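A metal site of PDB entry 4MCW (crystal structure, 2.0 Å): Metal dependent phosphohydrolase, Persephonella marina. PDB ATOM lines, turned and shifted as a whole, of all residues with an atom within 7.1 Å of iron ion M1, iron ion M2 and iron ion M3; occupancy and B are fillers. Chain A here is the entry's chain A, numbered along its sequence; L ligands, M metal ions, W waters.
NZ of Lys 231 touches iron ion M2, 3.6 Å away.
Of the 19 residues printed, 3 come within 4 Å of iron ion M2.
Iron ion M1 is bound by a ring nitrogen (NE2) of His 283, a ring nitrogen (NE2) of His 256, a ring nitrogen (NE2) of His 282, water W1, the side-chain carboxylate of Asp 228 and an oxygen (O4) of LIG L1.
Iron ion M1 has six donor atoms within binding distance.
Iron ion M2 is bound by water W1 (1.8 Å), OE1 of Glu 191 (2.0 Å), OD2 of Asp 228 (2.2 Å), O3 of LIG L1 (2.2 Å), O4 of LG2 L2 (2.2 Å) and water W2 (2.4 Å).
Iron ion M2 has six donor atoms within binding distance.
Of the 19 residues printed, 4 come within 4 Å of iron ion M1.
Residues that only touch iron ion M3: His 227 (3.7 Å).
Within 4 Å of iron ion M3: Glu 191, His 195, His 227 and Asp 311.
Water W2 lies within hydrogen-bond range of the side-chain carboxylate of Asp 311 and a ring nitrogen (NE2) of His 227.
Iron ion M3 is bound by water W2 (1.9 Å), NE2 of His 195 (2.0 Å), OE2 of Glu 191 (2.2 Å), N1 of LG3 L3 (2.2 Å), O3 of LG2 L2 (2.2 Å) and OD1 of Asp 311 (2.2 Å).
Iron ion M3 has six donor atoms within binding distance.
N of Glu 191 lies within hydrogen-bond range of OD1 of Asp 189, at 2.9 Å.
The side-chain carboxylate of Asp 228 lies close to the side-chain amino group of Lys 231 (3.2 Å).
A ring nitrogen (ND1) of His 282 sits at hydrogen-bond distance from the backbone carbonyl oxygen of Ala 279 (3.0 Å).
OE1 of Glu 191 sits close to NZ of Lys 231 (2.9 Å).
A ring nitrogen (ND1) of His 256 sits at hydrogen-bond distance from the backbone carbonyl oxygen (O) of Met 253, 2.9 Å away.
The side-chain hydroxyl of Tyr 291 lies within hydrogen-bond range of a ring nitrogen (ND1) of His 283 (3.0 Å).
OD2 of Asp 314 is in hydrogen-bond range of ND1 of His 195 (2.6 Å).
The side-chain amino group (NZ) of Lys 231 is in salt-bridge range of the side-chain carboxylate (OD2) of Asp 189 (3.0 Å).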
ATOM      1  N   ASP A 189     -16.988  10.891  10.505  1.00  0.00           N
ATOM      2  CA  ASP A 189     -17.839  10.959   9.307  1.00  0.00           C
ATOM      3  C   ASP A 189     -19.276  10.826   9.768  1.00  0.00           C
ATOM      4  O   ASP A 189     -19.543  10.092  10.700  1.00  0.00           O
ATOM      5  CB  ASP A 189     -17.463   9.878   8.304  1.00  0.00           C
ATOM      6  CG  ASP A 189     -18.303   9.915   7.034  1.00  0.00           C
ATOM      7  OD1 ASP A 189     -19.399   9.328   7.046  1.00  0.00           O
ATOM      8  OD2 ASP A 189     -17.861  10.517   6.020  1.00  0.00           O
ATOM      9  N   GLU A 191     -22.079   9.522   8.220  1.00  0.00           N
ATOM     10  CA  GLU A 191     -22.928   8.362   7.785  1.00  0.00           C
ATOM     11  C   GLU A 191     -23.295   7.510   9.011  1.00  0.00           C
ATOM     12  O   GLU A 191     -22.394   7.123   9.804  1.00  0.00           O
ATOM     13  CB  GLU A 191     -22.285   7.551   6.656  1.00  0.00           C
ATOM     14  CG  GLU A 191     -22.080   8.352   5.360  1.00  0.00           C
ATOM     15  CD  GLU A 191     -21.948   7.540   4.081  1.00  0.00           C
ATOM     16  OE1 GLU A 191     -21.237   7.980   3.125  1.00  0.00           O
ATOM     17  OE2 GLU A 191     -22.552   6.443   3.993  1.00  0.00           O
ATOM     18  N   HIS A 195     -28.044   3.746   8.401  1.00  0.00           N
ATOM     19  CA  HIS A 195     -27.822   3.910   6.973  1.00  0.00           C
ATOM     20  C   HIS A 195     -27.024   2.769   6.429  1.00  0.00           C
ATOM     21  O   HIS A 195     -27.338   2.211   5.365  1.00  0.00           O
ATOM     22  CB  HIS A 195     -27.140   5.240   6.725  1.00  0.00           C
ATOM     23  CG  HIS A 195     -26.521   5.348   5.370  1.00  0.00           C
ATOM     24  ND1 HIS A 195     -27.259   5.544   4.244  1.00  0.00           N
ATOM     25  CD2 HIS A 195     -25.193   5.323   4.975  1.00  0.00           C
ATOM     26  CE1 HIS A 195     -26.432   5.618   3.179  1.00  0.00           C
ATOM     27  NE2 HIS A 195     -25.162   5.530   3.638  1.00  0.00           N
ATOM     28  N   ILE A 196     -25.923   2.460   7.117  1.00  0.00           N
ATOM     29  CA  ILE A 196     -25.037   1.359   6.740  1.00  0.00           C
ATOM     30  C   ILE A 196     -25.805   0.019   6.674  1.00  0.00           C
ATOM     31  O   ILE A 196     -25.612  -0.729   5.748  1.00  0.00           O
ATOM     32  CB  ILE A 196     -23.849   1.291   7.752  1.00  0.00           C
ATOM     33  CG1 ILE A 196     -22.861   2.424   7.460  1.00  0.00           C
ATOM     34  CG2 ILE A 196     -23.190  -0.075   7.792  1.00  0.00           C
ATOM     35  CD1 ILE A 196     -22.006   2.778   8.680  1.00  0.00           C
ATOM     36  N   VAL A 199     -28.640   0.127   3.637  1.00  0.00           N
ATOM     37  CA  VAL A 199     -28.142   0.038   2.254  1.00  0.00           C
ATOM     38  C   VAL A 199     -27.924  -1.427   1.814  1.00  0.00           C
ATOM     39  O   VAL A 199     -28.226  -1.785   0.665  1.00  0.00           O
ATOM     40  CB  VAL A 199     -26.885   0.898   2.039  1.00  0.00           C
ATOM     41  CG1 VAL A 199     -26.245   0.641   0.694  1.00  0.00           C
ATOM     42  CG2 VAL A 199     -27.252   2.391   2.096  1.00  0.00           C
ATOM     43  N   HIS A 227     -18.751  -0.507   2.097  1.00  0.00           N
ATOM     44  CA  HIS A 227     -18.192   0.102   0.906  1.00  0.00           C
ATOM     45  C   HIS A 227     -17.434   1.392   1.196  1.00  0.00           C
ATOM     46  O   HIS A 227     -16.636   1.792   0.389  1.00  0.00           O
ATOM     47  CB  HIS A 227     -19.247   0.335  -0.194  1.00  0.00           C
ATOM     48  CG  HIS A 227     -20.283   1.373   0.154  1.00  0.00           C
ATOM     49  ND1 HIS A 227     -21.447   1.056   0.768  1.00  0.00           N
ATOM     50  CD2 HIS A 227     -20.285   2.762   0.012  1.00  0.00           C
ATOM     51  CE1 HIS A 227     -22.169   2.188   0.968  1.00  0.00           C
ATOM     52  NE2 HIS A 227     -21.454   3.232   0.507  1.00  0.00           N
ATOM     53  N   ASP A 228     -17.669   2.035   2.331  1.00  0.00           N
ATOM     54  CA  ASP A 228     -16.988   3.314   2.616  1.00  0.00           C
ATOM     55  C   ASP A 228     -15.875   3.195   3.649  1.00  0.00           C
ATOM     56  O   ASP A 228     -15.406   4.228   4.177  1.00  0.00           O
ATOM     57  CB  ASP A 228     -17.984   4.347   3.166  1.00  0.00           C
ATOM     58  CG  ASP A 228     -18.548   5.269   2.109  1.00  0.00           C
ATOM     59  OD1 ASP A 228     -18.068   5.403   0.962  1.00  0.00           O
ATOM     60  OD2 ASP A 228     -19.503   5.934   2.477  1.00  0.00           O
ATOM     61  N   LYS A 231     -12.627   5.372   4.043  1.00  0.00           N
ATOM     62  CA  LYS A 231     -12.591   6.718   4.622  1.00  0.00           C
ATOM     63  C   LYS A 231     -11.607   6.785   5.813  1.00  0.00           C
ATOM     64  O   LYS A 231     -11.090   7.862   6.127  1.00  0.00           O
ATOM     65  CB  LYS A 231     -13.983   7.163   5.060  1.00  0.00           C
ATOM     66  CG  LYS A 231     -14.861   7.537   3.873  1.00  0.00           C
ATOM     67  CD  LYS A 231     -16.166   8.113   4.371  1.00  0.00           C
ATOM     68  CE  LYS A 231     -17.088   8.471   3.197  1.00  0.00           C
ATOM     69  NZ  LYS A 231     -18.479   8.655   3.707  1.00  0.00           N
ATOM     70  N   MET A 253     -10.069  12.752  -1.432  1.00  0.00           N
ATOM     71  CA  MET A 253     -11.318  12.193  -0.927  1.00  0.00           C
ATOM     72  C   MET A 253     -11.793  11.020  -1.799  1.00  0.00           C
ATOM     73  O   MET A 253     -12.278  10.020  -1.290  1.00  0.00           O
ATOM     74  CB  MET A 253     -12.420  13.259  -0.839  1.00  0.00           C
ATOM     75  CG  MET A 253     -13.669  12.751  -0.169  1.00  0.00           C
ATOM     76  SD  MET A 253     -13.388  12.427   1.585  1.00  0.00           S
ATOM     77  CE  MET A 253     -14.541  11.082   1.862  1.00  0.00           C
ATOM     78  N   HIS A 256     -10.906   7.201  -1.288  1.00  0.00           N
ATOM     79  CA  HIS A 256     -11.498   6.315  -0.267  1.00  0.00           C
ATOM     80  C   HIS A 256     -11.997   5.044  -0.920  1.00  0.00           C
ATOM     81  O   HIS A 256     -12.149   4.025  -0.249  1.00  0.00           O
ATOM     82  CB  HIS A 256     -12.591   6.977   0.538  1.00  0.00           C
ATOM     83  CG  HIS A 256     -13.945   7.044  -0.177  1.00  0.00           C
ATOM     84  ND1 HIS A 256     -14.193   7.908  -1.180  1.00  0.00           N
ATOM     85  CD2 HIS A 256     -15.115   6.305   0.008  1.00  0.00           C
ATOM     86  CE1 HIS A 256     -15.448   7.743  -1.615  1.00  0.00           C
ATOM     87  NE2 HIS A 256     -16.013   6.752  -0.888  1.00  0.00           N
ATOM     88  N   THR A 257     -12.209   5.088  -2.238  1.00  0.00           N
ATOM     89  CA  THR A 257     -12.618   3.917  -2.998  1.00  0.00           C
ATOM     90  C   THR A 257     -11.462   2.896  -3.093  1.00  0.00           C
ATOM     91  O   THR A 257     -11.637   1.708  -2.762  1.00  0.00           O
ATOM     92  CB  THR A 257     -13.103   4.315  -4.410  1.00  0.00           C
ATOM     93  OG1 THR A 257     -12.054   5.028  -5.085  1.00  0.00           O
ATOM     94  CG2 THR A 257     -14.369   5.209  -4.307  1.00  0.00           C
ATOM     95  N   ALA A 279     -16.439  -1.536  -2.744  1.00  0.00           N
ATOM     96  CA  ALA A 279     -15.691  -0.415  -2.189  1.00  0.00           C
ATOM     97  C   ALA A 279     -15.063   0.377  -3.322  1.00  0.00           C
ATOM     98  O   ALA A 279     -15.144   1.605  -3.349  1.00  0.00           O
ATOM     99  CB  ALA A 279     -14.635  -0.870  -1.165  1.00  0.00           C
ATOM    100  N   HIS A 282     -18.382   1.791  -6.182  1.00  0.00           N
ATOM    101  CA  HIS A 282     -19.657   2.373  -5.850  1.00  0.00           C
ATOM    102  C   HIS A 282     -19.868   3.817  -6.317  1.00  0.00           C
ATOM    103  O   HIS A 282     -20.990   4.280  -6.282  1.00  0.00           O
ATOM    104  CB  HIS A 282     -20.024   2.165  -4.392  1.00  0.00           C
ATOM    105  CG  HIS A 282     -19.197   2.975  -3.429  1.00  0.00           C
ATOM    106  ND1 HIS A 282     -17.941   2.597  -3.050  1.00  0.00           N
ATOM    107  CD2 HIS A 282     -19.469   4.165  -2.774  1.00  0.00           C
ATOM    108  CE1 HIS A 282     -17.442   3.516  -2.195  1.00  0.00           C
ATOM    109  NE2 HIS A 282     -18.365   4.469  -2.019  1.00  0.00           N
ATOM    110  N   HIS A 283     -18.803   4.507  -6.767  1.00  0.00           N
ATOM    111  CA  HIS A 283     -18.950   5.863  -7.332  1.00  0.00           C
ATOM    112  C   HIS A 283     -18.786   5.833  -8.823  1.00  0.00           C
ATOM    113  O   HIS A 283     -18.768   6.868  -9.452  1.00  0.00           O
ATOM    114  CB  HIS A 283     -17.962   6.896  -6.693  1.00  0.00           C
ATOM    115  CG  HIS A 283     -18.226   7.149  -5.222  1.00  0.00           C
ATOM    116  ND1 HIS A 283     -19.204   7.969  -4.796  1.00  0.00           N
ATOM    117  CD2 HIS A 283     -17.605   6.644  -4.070  1.00  0.00           C
ATOM    118  CE1 HIS A 283     -19.221   7.972  -3.419  1.00  0.00           C
ATOM    119  NE2 HIS A 283     -18.224   7.161  -2.990  1.00  0.00           N
ATOM    120  N   TYR A 291     -16.199   7.895 -10.792  1.00  0.00           N
ATOM    121  CA  TYR A 291     -14.812   7.723 -10.358  1.00  0.00           C
ATOM    122  C   TYR A 291     -14.633   6.444  -9.534  1.00  0.00           C
ATOM    123  O   TYR A 291     -15.623   5.906  -8.998  1.00  0.00           O
ATOM    124  CB  TYR A 291     -14.338   8.957  -9.580  1.00  0.00           C
ATOM    125  CG  TYR A 291     -15.135   9.283  -8.310  1.00  0.00           C
ATOM    126  CD1 TYR A 291     -16.253  10.108  -8.374  1.00  0.00           C
ATOM    127  CD2 TYR A 291     -14.744   8.795  -7.064  1.00  0.00           C
ATOM    128  CE1 TYR A 291     -16.963  10.434  -7.227  1.00  0.00           C
ATOM    129  CE2 TYR A 291     -15.449   9.120  -5.903  1.00  0.00           C
ATOM    130  CZ  TYR A 291     -16.559   9.934  -6.008  1.00  0.00           C
ATOM    131  OH  TYR A 291     -17.297  10.283  -4.888  1.00  0.00           O
ATOM    132  N   ASP A 311     -27.619   3.186  -2.120  1.00  0.00           N
ATOM    133  CA  ASP A 311     -26.975   4.249  -1.334  1.00  0.00           C
ATOM    134  C   ASP A 311     -27.593   5.620  -1.692  1.00  0.00           C
ATOM    135  O   ASP A 311     -27.937   6.375  -0.822  1.00  0.00           O
ATOM    136  CB  ASP A 311     -25.493   4.246  -1.674  1.00  0.00           C
ATOM    137  CG  ASP A 311     -24.677   5.048  -0.670  1.00  0.00           C
ATOM    138  OD1 ASP A 311     -24.840   4.896   0.562  1.00  0.00           O
ATOM    139  OD2 ASP A 311     -23.868   5.859  -1.124  1.00  0.00           O
ATOM    140  N   VAL A 312     -27.717   5.925  -2.969  1.00  0.00           N
ATOM    141  CA  VAL A 312     -28.434   7.167  -3.404  1.00  0.00           C
ATOM    142  C   VAL A 312     -29.880   7.195  -2.890  1.00  0.00           C
ATOM    143  O   VAL A 312     -30.342   8.236  -2.403  1.00  0.00           O
ATOM    144  CB  VAL A 312     -28.357   7.348  -4.919  1.00  0.00           C
ATOM    145  CG1 VAL A 312     -29.165   8.580  -5.378  1.00  0.00           C
ATOM    146  CG2 VAL A 312     -26.910   7.501  -5.353  1.00  0.00           C
ATOM    147  N   ASP A 314     -31.122   5.832  -0.235  1.00  0.00           N
ATOM    148  CA  ASP A 314     -31.156   6.119   1.195  1.00  0.00           C
ATOM    149  C   ASP A 314     -30.888   7.598   1.446  1.00  0.00           C
ATOM    150  O   ASP A 314     -31.516   8.196   2.324  1.00  0.00           O
ATOM    151  CB  ASP A 314     -30.172   5.249   2.048  1.00  0.00           C
ATOM    152  CG  ASP A 314     -30.630   5.153   3.486  1.00  0.00           C
ATOM    153  OD1 ASP A 314     -31.812   4.818   3.719  1.00  0.00           O
ATOM    154  OD2 ASP A 314     -29.859   5.436   4.419  1.00  0.00           O
ATOM    155  N   ALA A 315     -29.996   8.188   0.675  1.00  0.00           N
ATOM    156  CA  ALA A 315     -29.639   9.606   0.874  1.00  0.00           C
ATOM    157  C   ALA A 315     -30.779  10.545   0.443  1.00  0.00           C
ATOM    158  O   ALA A 315     -31.058  11.494   1.143  1.00  0.00           O
ATOM    159  CB  ALA A 315     -28.358   9.949   0.129  1.00  0.00           C
HETATM  160  C1  LIG L   1     -17.512  11.025  -2.013  1.00  0.00           C
HETATM  161  O1  LIG L   1     -16.579  10.694  -2.807  1.00  0.00           O
HETATM  162  O2  LIG L   1     -18.709  11.255  -2.386  1.00  0.00           O
HETATM  163  C2  LIG L   1     -17.113  11.130  -0.563  1.00  0.00           C
HETATM  164  C3  LIG L   1     -18.236  10.869   0.440  1.00  0.00           C
HETATM  165  C4  LIG L   1     -18.594   9.391   0.470  1.00  0.00           C
HETATM  166  O3  LIG L   1     -19.437   8.997   1.298  1.00  0.00           O
HETATM  167  O4  LIG L   1     -18.042   8.611  -0.325  1.00  0.00           O
HETATM  168  C1  LG2 L   2     -25.467  10.606  -1.868  1.00  0.00           C
HETATM  169  O1  LG2 L   2     -25.877  10.523  -3.032  1.00  0.00           O
HETATM  170  O2  LG2 L   2     -25.663  11.637  -1.175  1.00  0.00           O
HETATM  171  C2  LG2 L   2     -24.692   9.419  -1.271  1.00  0.00           C
HETATM  172  C3  LG2 L   2     -24.468   9.615   0.230  1.00  0.00           C
HETATM  173  C4  LG2 L   2     -23.554   8.542   0.846  1.00  0.00           C
HETATM  174  O3  LG2 L   2     -23.975   7.796   1.767  1.00  0.00           O
HETATM  175  O4  LG2 L   2     -22.386   8.495   0.449  1.00  0.00           O
HETATM  176  N1  LG3 L   3     -22.957   3.832   3.189  1.00  0.00           N
HETATM  177  C1  LG3 L   3     -21.679   3.612   3.558  1.00  0.00           C
HETATM  178  N2  LG3 L   3     -21.571   2.301   3.862  1.00  0.00           N
HETATM  179  C2  LG3 L   3     -22.770   1.696   3.698  1.00  0.00           C
HETATM  180  C3  LG3 L   3     -23.657   2.675   3.270  1.00  0.00           C
HETATM  181 FE    FE M   1     -18.108   6.373  -1.067  1.00  0.00          FE
HETATM  182 FE    FE M   2     -20.751   7.278   1.345  1.00  0.00          FE
HETATM  183 FE    FE M   3     -23.632   5.682   2.288  1.00  0.00          FE
HETATM  184  O   HOH W   1     -20.045   6.791  -0.199  1.00  0.00           O
HETATM  185  O   HOH W   2     -22.345   5.601   0.917  1.00  0.00           O
